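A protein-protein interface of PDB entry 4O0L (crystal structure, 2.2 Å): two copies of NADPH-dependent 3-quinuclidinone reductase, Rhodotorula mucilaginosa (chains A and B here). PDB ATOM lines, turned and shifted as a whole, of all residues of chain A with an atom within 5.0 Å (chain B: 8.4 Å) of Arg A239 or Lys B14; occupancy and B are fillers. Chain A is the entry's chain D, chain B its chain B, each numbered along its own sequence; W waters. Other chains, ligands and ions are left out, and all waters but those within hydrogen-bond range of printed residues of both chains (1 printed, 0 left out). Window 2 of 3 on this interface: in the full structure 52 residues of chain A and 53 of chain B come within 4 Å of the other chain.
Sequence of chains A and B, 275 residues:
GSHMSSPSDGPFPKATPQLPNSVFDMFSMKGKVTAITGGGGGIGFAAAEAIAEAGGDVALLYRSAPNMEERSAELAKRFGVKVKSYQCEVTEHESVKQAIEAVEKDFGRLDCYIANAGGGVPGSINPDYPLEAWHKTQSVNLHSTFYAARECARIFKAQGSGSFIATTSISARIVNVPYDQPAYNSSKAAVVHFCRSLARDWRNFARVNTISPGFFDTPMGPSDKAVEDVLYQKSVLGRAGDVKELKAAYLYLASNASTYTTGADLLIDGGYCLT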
ATOM      1  N   LEU A 231      -1.130  27.703 -13.623  1.00  0.00           N
ATOM      2  CA  LEU A 231      -2.046  27.219 -12.602  1.00  0.00           C
ATOM      3  C   LEU A 231      -3.347  26.659 -13.199  1.00  0.00           C
ATOM      4  O   LEU A 231      -3.811  25.592 -12.787  1.00  0.00           O
ATOM      5  CB  LEU A 231      -2.336  28.347 -11.605  1.00  0.00           C
ATOM      6  CG  LEU A 231      -3.017  28.177 -10.221  1.00  0.00           C
ATOM      7  CD1 LEU A 231      -4.360  28.890 -10.236  1.00  0.00           C
ATOM      8  CD2 LEU A 231      -3.109  26.748  -9.690  1.00  0.00           C
ATOM      9  N   TYR A 232      -3.917  27.346 -14.183  1.00  0.00           N
ATOM     10  CA  TYR A 232      -5.200  26.913 -14.778  1.00  0.00           C
ATOM     11  C   TYR A 232      -5.028  25.616 -15.554  1.00  0.00           C
ATOM     12  O   TYR A 232      -5.924  24.763 -15.553  1.00  0.00           O
ATOM     13  CB  TYR A 232      -5.849  28.020 -15.627  1.00  0.00           C
ATOM     14  CG  TYR A 232      -6.038  29.303 -14.855  1.00  0.00           C
ATOM     15  CD1 TYR A 232      -6.282  29.281 -13.477  1.00  0.00           C
ATOM     16  CD2 TYR A 232      -5.969  30.547 -15.490  1.00  0.00           C
ATOM     17  CE1 TYR A 232      -6.427  30.444 -12.744  1.00  0.00           C
ATOM     18  CE2 TYR A 232      -6.130  31.740 -14.760  1.00  0.00           C
ATOM     19  CZ  TYR A 232      -6.352  31.677 -13.391  1.00  0.00           C
ATOM     20  OH  TYR A 232      -6.498  32.830 -12.626  1.00  0.00           O
ATOM     21  N   SER A 235      -3.530  22.766 -12.081  1.00  0.00           N
ATOM     22  CA  SER A 235      -4.588  22.441 -11.119  1.00  0.00           C
ATOM     23  C   SER A 235      -5.736  21.834 -11.918  1.00  0.00           C
ATOM     24  O   SER A 235      -6.202  22.440 -12.887  1.00  0.00           O
ATOM     25  CB  SER A 235      -5.050  23.699 -10.387  1.00  0.00           C
ATOM     26  OG  SER A 235      -6.079  23.410  -9.444  1.00  0.00           O
ATOM     27  N   LEU A 237      -8.661  21.449 -10.922  1.00  0.00           N
ATOM     28  CA  LEU A 237      -9.820  22.270 -10.565  1.00  0.00           C
ATOM     29  C   LEU A 237      -9.823  23.625 -11.278  1.00  0.00           C
ATOM     30  O   LEU A 237     -10.804  24.348 -11.187  1.00  0.00           O
ATOM     31  CB  LEU A 237      -9.887  22.479  -9.042  1.00  0.00           C
ATOM     32  CG  LEU A 237     -10.699  21.514  -8.202  1.00  0.00           C
ATOM     33  CD1 LEU A 237     -10.814  20.127  -8.787  1.00  0.00           C
ATOM     34  CD2 LEU A 237     -10.177  21.442  -6.753  1.00  0.00           C
ATOM     35  N   GLY A 238      -8.726  23.951 -11.964  1.00  0.00           N
ATOM     36  CA  GLY A 238      -8.629  25.153 -12.796  1.00  0.00           C
ATOM     37  C   GLY A 238      -8.782  26.507 -12.108  1.00  0.00           C
ATOM     38  O   GLY A 238      -9.321  27.476 -12.684  1.00  0.00           O
ATOM     39  N   ARG A 239      -8.290  26.588 -10.880  1.00  0.00           N
ATOM     40  CA  ARG A 239      -8.403  27.795 -10.074  1.00  0.00           C
ATOM     41  C   ARG A 239      -7.410  27.738  -8.924  1.00  0.00           C
ATOM     42  O   ARG A 239      -6.844  26.674  -8.632  1.00  0.00           O
ATOM     43  CB  ARG A 239      -9.821  27.945  -9.520  1.00  0.00           C
ATOM     44  CG  ARG A 239     -10.225  26.816  -8.577  1.00  0.00           C
ATOM     45  CD  ARG A 239     -11.517  27.114  -7.910  1.00  0.00           C
ATOM     46  NE  ARG A 239     -11.910  25.996  -7.080  1.00  0.00           N
ATOM     47  CZ  ARG A 239     -11.625  25.867  -5.797  1.00  0.00           C
ATOM     48  NH1 ARG A 239     -12.017  24.793  -5.153  1.00  0.00           N
ATOM     49  NH2 ARG A 239     -10.910  26.797  -5.164  1.00  0.00           N
ATOM     50  N   ALA A 240      -7.170  28.896  -8.311  1.00  0.00           N
ATOM     51  CA  ALA A 240      -6.378  28.990  -7.088  1.00  0.00           C
ATOM     52  C   ALA A 240      -7.283  28.580  -5.914  1.00  0.00           C
ATOM     53  O   ALA A 240      -8.508  28.705  -5.988  1.00  0.00           O
ATOM     54  CB  ALA A 240      -5.878  30.406  -6.894  1.00  0.00           C
ATOM     55  N   GLY A 241      -6.671  28.106  -4.850  1.00  0.00           N
ATOM     56  CA  GLY A 241      -7.415  27.790  -3.644  1.00  0.00           C
ATOM     57  C   GLY A 241      -7.894  29.060  -2.928  1.00  0.00           C
ATOM     58  O   GLY A 241      -7.352  30.135  -3.114  1.00  0.00           O
ATOM     59  N   ASP A 242      -8.914  28.906  -2.098  1.00  0.00           N
ATOM     60  CA  ASP A 242      -9.353  29.945  -1.208  1.00  0.00           C
ATOM     61  C   ASP A 242      -8.949  29.466   0.202  1.00  0.00           C
ATOM     62  O   ASP A 242      -9.200  28.344   0.545  1.00  0.00           O
ATOM     63  CB  ASP A 242     -10.874  30.144  -1.350  1.00  0.00           C
ATOM     64  CG  ASP A 242     -11.457  31.120  -0.326  1.00  0.00           C
ATOM     65  OD1 ASP A 242     -11.353  30.906   0.904  1.00  0.00           O
ATOM     66  OD2 ASP A 242     -12.043  32.109  -0.760  1.00  0.00           O
ATOM     67  N   GLU A 245     -10.342  26.698   2.390  1.00  0.00           N
ATOM     68  CA  GLU A 245     -10.094  25.338   1.997  1.00  0.00           C
ATOM     69  C   GLU A 245      -8.842  24.712   2.673  1.00  0.00           C
ATOM     70  O   GLU A 245      -8.561  23.533   2.469  1.00  0.00           O
ATOM     71  CB  GLU A 245      -9.997  25.251   0.466  1.00  0.00           C
ATOM     72  CG  GLU A 245     -11.275  25.653  -0.274  1.00  0.00           C
ATOM     73  CD  GLU A 245     -11.114  25.690  -1.777  1.00  0.00           C
ATOM     74  OE1 GLU A 245     -11.726  24.848  -2.475  1.00  0.00           O
ATOM     75  OE2 GLU A 245     -10.399  26.580  -2.265  1.00  0.00           O
ATOM     76  N   GLY B  10     -11.942  29.291 -23.031  1.00  0.00           N
ATOM     77  CA  GLY B  10     -11.492  30.016 -21.809  1.00  0.00           C
ATOM     78  C   GLY B  10     -12.575  30.137 -20.723  1.00  0.00           C
ATOM     79  O   GLY B  10     -13.137  31.222 -20.495  1.00  0.00           O
ATOM     80  N   PRO B  11     -12.890  29.017 -20.043  1.00  0.00           N
ATOM     81  CA  PRO B  11     -13.705  29.195 -18.869  1.00  0.00           C
ATOM     82  C   PRO B  11     -12.815  29.240 -17.605  1.00  0.00           C
ATOM     83  O   PRO B  11     -13.238  28.739 -16.556  1.00  0.00           O
ATOM     84  CB  PRO B  11     -14.607  27.942 -18.896  1.00  0.00           C
ATOM     85  CG  PRO B  11     -13.877  26.901 -19.746  1.00  0.00           C
ATOM     86  CD  PRO B  11     -12.622  27.582 -20.284  1.00  0.00           C
ATOM     87  N   PHE B  12     -11.611  29.834 -17.728  1.00  0.00           N
ATOM     88  CA  PHE B  12     -10.645  30.000 -16.615  1.00  0.00           C
ATOM     89  C   PHE B  12     -10.426  31.446 -16.154  1.00  0.00           C
ATOM     90  O   PHE B  12     -10.204  32.329 -16.989  1.00  0.00           O
ATOM     91  CB  PHE B  12      -9.271  29.403 -16.978  1.00  0.00           C
ATOM     92  CG  PHE B  12      -9.311  27.939 -17.265  1.00  0.00           C
ATOM     93  CD1 PHE B  12      -9.470  27.013 -16.226  1.00  0.00           C
ATOM     94  CD2 PHE B  12      -9.220  27.481 -18.581  1.00  0.00           C
ATOM     95  CE1 PHE B  12      -9.530  25.655 -16.514  1.00  0.00           C
ATOM     96  CE2 PHE B  12      -9.270  26.125 -18.865  1.00  0.00           C
ATOM     97  CZ  PHE B  12      -9.410  25.211 -17.841  1.00  0.00           C
ATOM     98  N   PRO B  13     -10.432  31.694 -14.825  1.00  0.00           N
ATOM     99  CA  PRO B  13     -10.548  30.664 -13.786  1.00  0.00           C
ATOM    100  C   PRO B  13     -11.996  30.211 -13.519  1.00  0.00           C
ATOM    101  O   PRO B  13     -12.988  30.950 -13.756  1.00  0.00           O
ATOM    102  CB  PRO B  13      -9.955  31.352 -12.536  1.00  0.00           C
ATOM    103  CG  PRO B  13     -10.247  32.824 -12.737  1.00  0.00           C
ATOM    104  CD  PRO B  13     -10.319  33.053 -14.247  1.00  0.00           C
ATOM    105  N   LYS B  14     -12.080  28.988 -13.036  1.00  0.00           N
ATOM    106  CA  LYS B  14     -13.336  28.294 -12.746  1.00  0.00           C
ATOM    107  C   LYS B  14     -13.773  28.855 -11.449  1.00  0.00           C
ATOM    108  O   LYS B  14     -12.891  29.264 -10.664  1.00  0.00           O
ATOM    109  CB  LYS B  14     -13.034  26.831 -12.498  1.00  0.00           C
ATOM    110  CG  LYS B  14     -13.394  25.930 -13.679  1.00  0.00           C
ATOM    111  CD  LYS B  14     -12.153  25.151 -14.144  1.00  0.00           C
ATOM    112  CE  LYS B  14     -12.596  24.051 -15.067  1.00  0.00           C
ATOM    113  NZ  LYS B  14     -13.884  24.519 -15.655  1.00  0.00           N
ATOM    114  N   ALA B  15     -15.082  28.894 -11.193  1.00  0.00           N
ATOM    115  CA  ALA B  15     -15.558  29.603 -10.003  1.00  0.00           C
ATOM    116  C   ALA B  15     -15.155  28.815  -8.765  1.00  0.00           C
ATOM    117  O   ALA B  15     -15.114  27.592  -8.785  1.00  0.00           O
ATOM    118  CB  ALA B  15     -17.078  29.787 -10.041  1.00  0.00           C
ATOM    119  N   THR B  16     -14.872  29.517  -7.678  1.00  0.00           N
ATOM    120  CA  THR B  16     -14.649  28.809  -6.440  1.00  0.00           C
ATOM    121  C   THR B  16     -16.014  28.377  -5.854  1.00  0.00           C
ATOM    122  O   THR B  16     -17.003  29.110  -5.952  1.00  0.00           O
ATOM    123  CB  THR B  16     -13.701  29.588  -5.493  1.00  0.00           C
ATOM    124  OG1 THR B  16     -14.146  29.465  -4.126  1.00  0.00           O
ATOM    125  CG2 THR B  16     -13.557  31.017  -5.894  1.00  0.00           C
ATOM    126  N   PRO B  17     -16.087  27.149  -5.312  1.00  0.00           N
ATOM    127  CA  PRO B  17     -17.355  26.637  -4.846  1.00  0.00           C
ATOM    128  C   PRO B  17     -17.918  27.482  -3.714  1.00  0.00           C
ATOM    129  O   PRO B  17     -17.279  28.408  -3.261  1.00  0.00           O
ATOM    130  CB  PRO B  17     -17.012  25.215  -4.357  1.00  0.00           C
ATOM    131  CG  PRO B  17     -15.564  25.317  -3.968  1.00  0.00           C
ATOM    132  CD  PRO B  17     -14.997  26.178  -5.076  1.00  0.00           C
ATOM    133  N   GLN B  18     -19.136  27.151  -3.308  1.00  0.00           N
ATOM    134  CA  GLN B  18     -19.740  27.753  -2.133  1.00  0.00           C
ATOM    135  C   GLN B  18     -19.013  27.224  -0.925  1.00  0.00           C
ATOM    136  O   GLN B  18     -19.073  26.028  -0.632  1.00  0.00           O
ATOM    137  CB  GLN B  18     -21.234  27.416  -2.062  1.00  0.00           C
ATOM    138  CG  GLN B  18     -21.945  28.021  -0.840  1.00  0.00           C
ATOM    139  CD  GLN B  18     -21.950  29.537  -0.869  1.00  0.00           C
ATOM    140  OE1 GLN B  18     -21.872  30.159  -1.949  1.00  0.00           O
ATOM    141  NE2 GLN B  18     -22.043  30.148   0.296  1.00  0.00           N
ATOM    142  N   LEU B  19     -18.328  28.115  -0.222  1.00  0.00           N
ATOM    143  CA  LEU B  19     -17.475  27.743   0.901  1.00  0.00           C
ATOM    144  C   LEU B  19     -17.990  28.268   2.229  1.00  0.00           C
ATOM    145  O   LEU B  19     -17.957  29.466   2.464  1.00  0.00           O
ATOM    146  CB  LEU B  19     -16.037  28.221   0.649  1.00  0.00           C
ATOM    147  CG  LEU B  19     -15.335  27.502  -0.503  1.00  0.00           C
ATOM    148  CD1 LEU B  19     -14.084  28.225  -0.904  1.00  0.00           C
ATOM    149  CD2 LEU B  19     -15.003  26.043  -0.164  1.00  0.00           C
ATOM    150  N   ARG B 203     -12.181  15.572 -12.832  1.00  0.00           N
ATOM    151  CA  ARG B 203     -11.947  16.890 -12.280  1.00  0.00           C
ATOM    152  C   ARG B 203     -13.121  17.870 -12.401  1.00  0.00           C
ATOM    153  O   ARG B 203     -13.196  18.820 -11.609  1.00  0.00           O
ATOM    154  CB  ARG B 203     -10.720  17.515 -12.934  1.00  0.00           C
ATOM    155  CG  ARG B 203     -10.943  17.945 -14.376  1.00  0.00           C
ATOM    156  CD  ARG B 203      -9.649  18.133 -15.118  1.00  0.00           C
ATOM    157  NE  ARG B 203      -9.875  18.335 -16.548  1.00  0.00           N
ATOM    158  CZ  ARG B 203     -10.171  17.393 -17.415  1.00  0.00           C
ATOM    159  NH1 ARG B 203     -10.372  17.705 -18.679  1.00  0.00           N
ATOM    160  NH2 ARG B 203     -10.261  16.140 -17.028  1.00  0.00           N
ATOM    161  N   ASN B 204     -14.011  17.664 -13.371  1.00  0.00           N
ATOM    162  CA  ASN B 204     -15.164  18.579 -13.545  1.00  0.00           C
ATOM    163  C   ASN B 204     -16.371  18.252 -12.701  1.00  0.00           C
ATOM    164  O   ASN B 204     -17.337  19.007 -12.696  1.00  0.00           O
ATOM    165  CB  ASN B 204     -15.565  18.652 -15.029  1.00  0.00           C
ATOM    166  CG  ASN B 204     -14.533  19.359 -15.882  1.00  0.00           C
ATOM    167  OD1 ASN B 204     -13.970  20.349 -15.484  1.00  0.00           O
ATOM    168  ND2 ASN B 204     -14.298  18.850 -17.044  1.00  0.00           N
ATOM    169  N   ARG B 207     -14.024  14.895  -6.587  1.00  0.00           N
ATOM    170  CA  ARG B 207     -12.698  14.800  -5.989  1.00  0.00           C
ATOM    171  C   ARG B 207     -12.378  13.334  -5.687  1.00  0.00           C
ATOM    172  O   ARG B 207     -13.283  12.534  -5.485  1.00  0.00           O
ATOM    173  CB  ARG B 207     -12.575  15.649  -4.718  1.00  0.00           C
ATOM    174  CG  ARG B 207     -12.667  17.142  -4.959  1.00  0.00           C
ATOM    175  CD  ARG B 207     -12.608  17.947  -3.668  1.00  0.00           C
ATOM    176  NE  ARG B 207     -13.685  17.587  -2.735  1.00  0.00           N
ATOM    177  CZ  ARG B 207     -13.540  16.864  -1.638  1.00  0.00           C
ATOM    178  NH1 ARG B 207     -12.342  16.366  -1.295  1.00  0.00           N
ATOM    179  NH2 ARG B 207     -14.593  16.637  -0.869  1.00  0.00           N
ATOM    180  N   SER B 258     -12.676  19.653   2.561  1.00  0.00           N
ATOM    181  CA  SER B 258     -11.517  19.345   1.705  1.00  0.00           C
ATOM    182  C   SER B 258     -11.684  19.661   0.227  1.00  0.00           C
ATOM    183  O   SER B 258     -11.121  18.963  -0.601  1.00  0.00           O
ATOM    184  CB  SER B 258     -11.113  17.897   1.867  1.00  0.00           C
ATOM    185  OG  SER B 258     -12.168  17.007   1.529  1.00  0.00           O
ATOM    186  N   THR B 259     -12.402  20.741  -0.101  1.00  0.00           N
ATOM    187  CA  THR B 259     -12.774  21.046  -1.489  1.00  0.00           C
ATOM    188  C   THR B 259     -11.611  21.349  -2.448  1.00  0.00           C
ATOM    189  O   THR B 259     -11.790  21.239  -3.664  1.00  0.00           O
ATOM    190  CB  THR B 259     -13.776  22.237  -1.563  1.00  0.00           C
ATOM    191  OG1 THR B 259     -13.217  23.348  -0.852  1.00  0.00           O
ATOM    192  CG2 THR B 259     -15.098  21.843  -0.961  1.00  0.00           C
ATOM    193  N   TYR B 260     -10.451  21.729  -1.928  1.00  0.00           N
ATOM    194  CA  TYR B 260      -9.272  21.925  -2.781  1.00  0.00           C
ATOM    195  C   TYR B 260      -8.297  20.743  -2.669  1.00  0.00           C
ATOM    196  O   TYR B 260      -7.152  20.787  -3.194  1.00  0.00           O
ATOM    197  CB  TYR B 260      -8.568  23.235  -2.466  1.00  0.00           C
ATOM    198  CG  TYR B 260      -7.743  23.839  -3.600  1.00  0.00           C
ATOM    199  CD1 TYR B 260      -8.331  24.192  -4.803  1.00  0.00           C
ATOM    200  CD2 TYR B 260      -6.391  24.098  -3.424  1.00  0.00           C
ATOM    201  CE1 TYR B 260      -7.570  24.774  -5.839  1.00  0.00           C
ATOM    202  CE2 TYR B 260      -5.627  24.665  -4.411  1.00  0.00           C
ATOM    203  CZ  TYR B 260      -6.201  24.994  -5.627  1.00  0.00           C
ATOM    204  OH  TYR B 260      -5.434  25.563  -6.597  1.00  0.00           O
ATOM    205  N   THR B 261      -8.761  19.679  -2.016  1.00  0.00           N
ATOM    206  CA  THR B 261      -7.931  18.478  -1.812  1.00  0.00           C
ATOM    207  C   THR B 261      -8.348  17.389  -2.785  1.00  0.00           C
ATOM    208  O   THR B 261      -9.407  16.752  -2.621  1.00  0.00           O
ATOM    209  CB  THR B 261      -8.044  17.923  -0.375  1.00  0.00           C
ATOM    210  OG1 THR B 261      -7.913  18.997   0.569  1.00  0.00           O
ATOM    211  CG2 THR B 261      -6.918  16.881  -0.115  1.00  0.00           C
HETATM  212  O   HOH W   1      -9.249  21.406   0.664  1.00  0.00           O
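The backbone NH of Lys B14 is in hydrogen-bond range of the backbone carbonyl oxygen of Gly A238 (3.2 Å).
The side-chain hydroxyl (OG1) of Thr B259 is in hydrogen-bond range of the side-chain carboxylate (OE1) of Glu A245 (2.7 Å).
The backbone carbonyl oxygen of Arg A239 sits at hydrogen-bond distance from the side-chain hydroxyl of Tyr B260 (2.7 Å).
The side-chain hydroxyl (OH) of Tyr B260 sits close to the backbone NH (N) of Gly A241.
The backbone NH (N) of Tyr B260 is in hydrogen-bond range of the side-chain carboxylate (OE1) of Glu A245, 3.4 Å away.
OG of Ser A235 lies within hydrogen-bond range of O of Arg A239, 3.4 Å away.
The side-chain carboxylate (OE1) of Glu A245 lies within salt-bridge range of the guanidinium group (NH1) of Arg A239, at 2.7 Å.
The backbone NH of Asp A242 is in hydrogen-bond range of the side-chain carboxylate of Glu A245.
Tyr B260 touches Ser A235 (OH to OG, 3.6 Å).
O of Leu A237 touches CD of Lys B14, at 3.3 Å.
CD2 of Leu A237 touches O of Thr B259 (3.5 Å).
Leu A237 touches Tyr B260 (CD2 to CD1, 3.8 Å).
Phe B12 touches Gly A238 (CD1 to O, 3.6 Å).
Pro B13 touches Gly A238.
Ala B15 touches Arg A239 (O to CD, 3.7 Å).
Arg A239 touches Thr B16 (CD to CA, 3.9 Å).
Arg A239 touches Thr B259.
CD1 of Leu B19 touches CB of Asp A242, 3.8 Å away.
Of the printed residues of chain B, Leu A237 touches Lys B14, Arg B203, Thr B259 and Tyr B260.
Gly A238 touches just these residues of chain B: Phe B12 (3.6 Å), Pro B13 (3.6 Å) and Lys B14 (3.2 Å).
Printed residues of chain B within 4 Å of Arg A239: Lys B14, Ala B15, Thr B16, Pro B17, Thr B259 and Tyr B260.
Of the printed residues of chain B, Gly A241 touches Tyr B260 (3.2 Å).
Of the printed residues of chain B, Glu A245 touches Leu B19 (3.7 Å), Thr B259 (2.7 Å) and Tyr B260 (3.4 Å).
Of the printed residues of chain A, Phe B12 touches Tyr A232 (3.8 Å) and Gly A238 (3.6 Å).
Lys B14 touches just these residues of chain A: Leu A237, Gly A238 and Arg A239.
Of the printed residues of chain A, Arg B203 touches Leu A237 (3.9 Å).
The nearest printed residue of chain A that does not touch Pro B17 is Glu A245 (4.1 Å).
Of the 17 printed residues of chain B, 10 touch a printed residue of chain A.
Hydrophobic or aromatic side chains of chain B within 4 Å of the printed part of chain A: Phe B12, Pro B13, Pro B17, Leu B19 and Tyr B260.
Along chain B the printed residues that touch a printed residue of chain A span positions 12 to 260.
Among the printed residues, no Asp or Glu carboxylate lies within 4 Å of a Lys or Arg side-chain nitrogen of the other chain.
No position is printed for both chains.
Of the 22 pairs that touch across the chains among the printed residues, none has its exchanged pair printed and touching as well.
Water W1 lies within hydrogen-bond range of the side-chain hydroxyl (OG1) of Thr B261 (2.8 Å), the backbone carbonyl oxygen (O) of Glu A245 (2.9 Å), the backbone NH (N) of Tyr B260 (2.9 Å), the backbone NH (N) of Thr B259 (3.3 Å) and the backbone carbonyl oxygen (O) of Ser B258 (3.3 Å).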
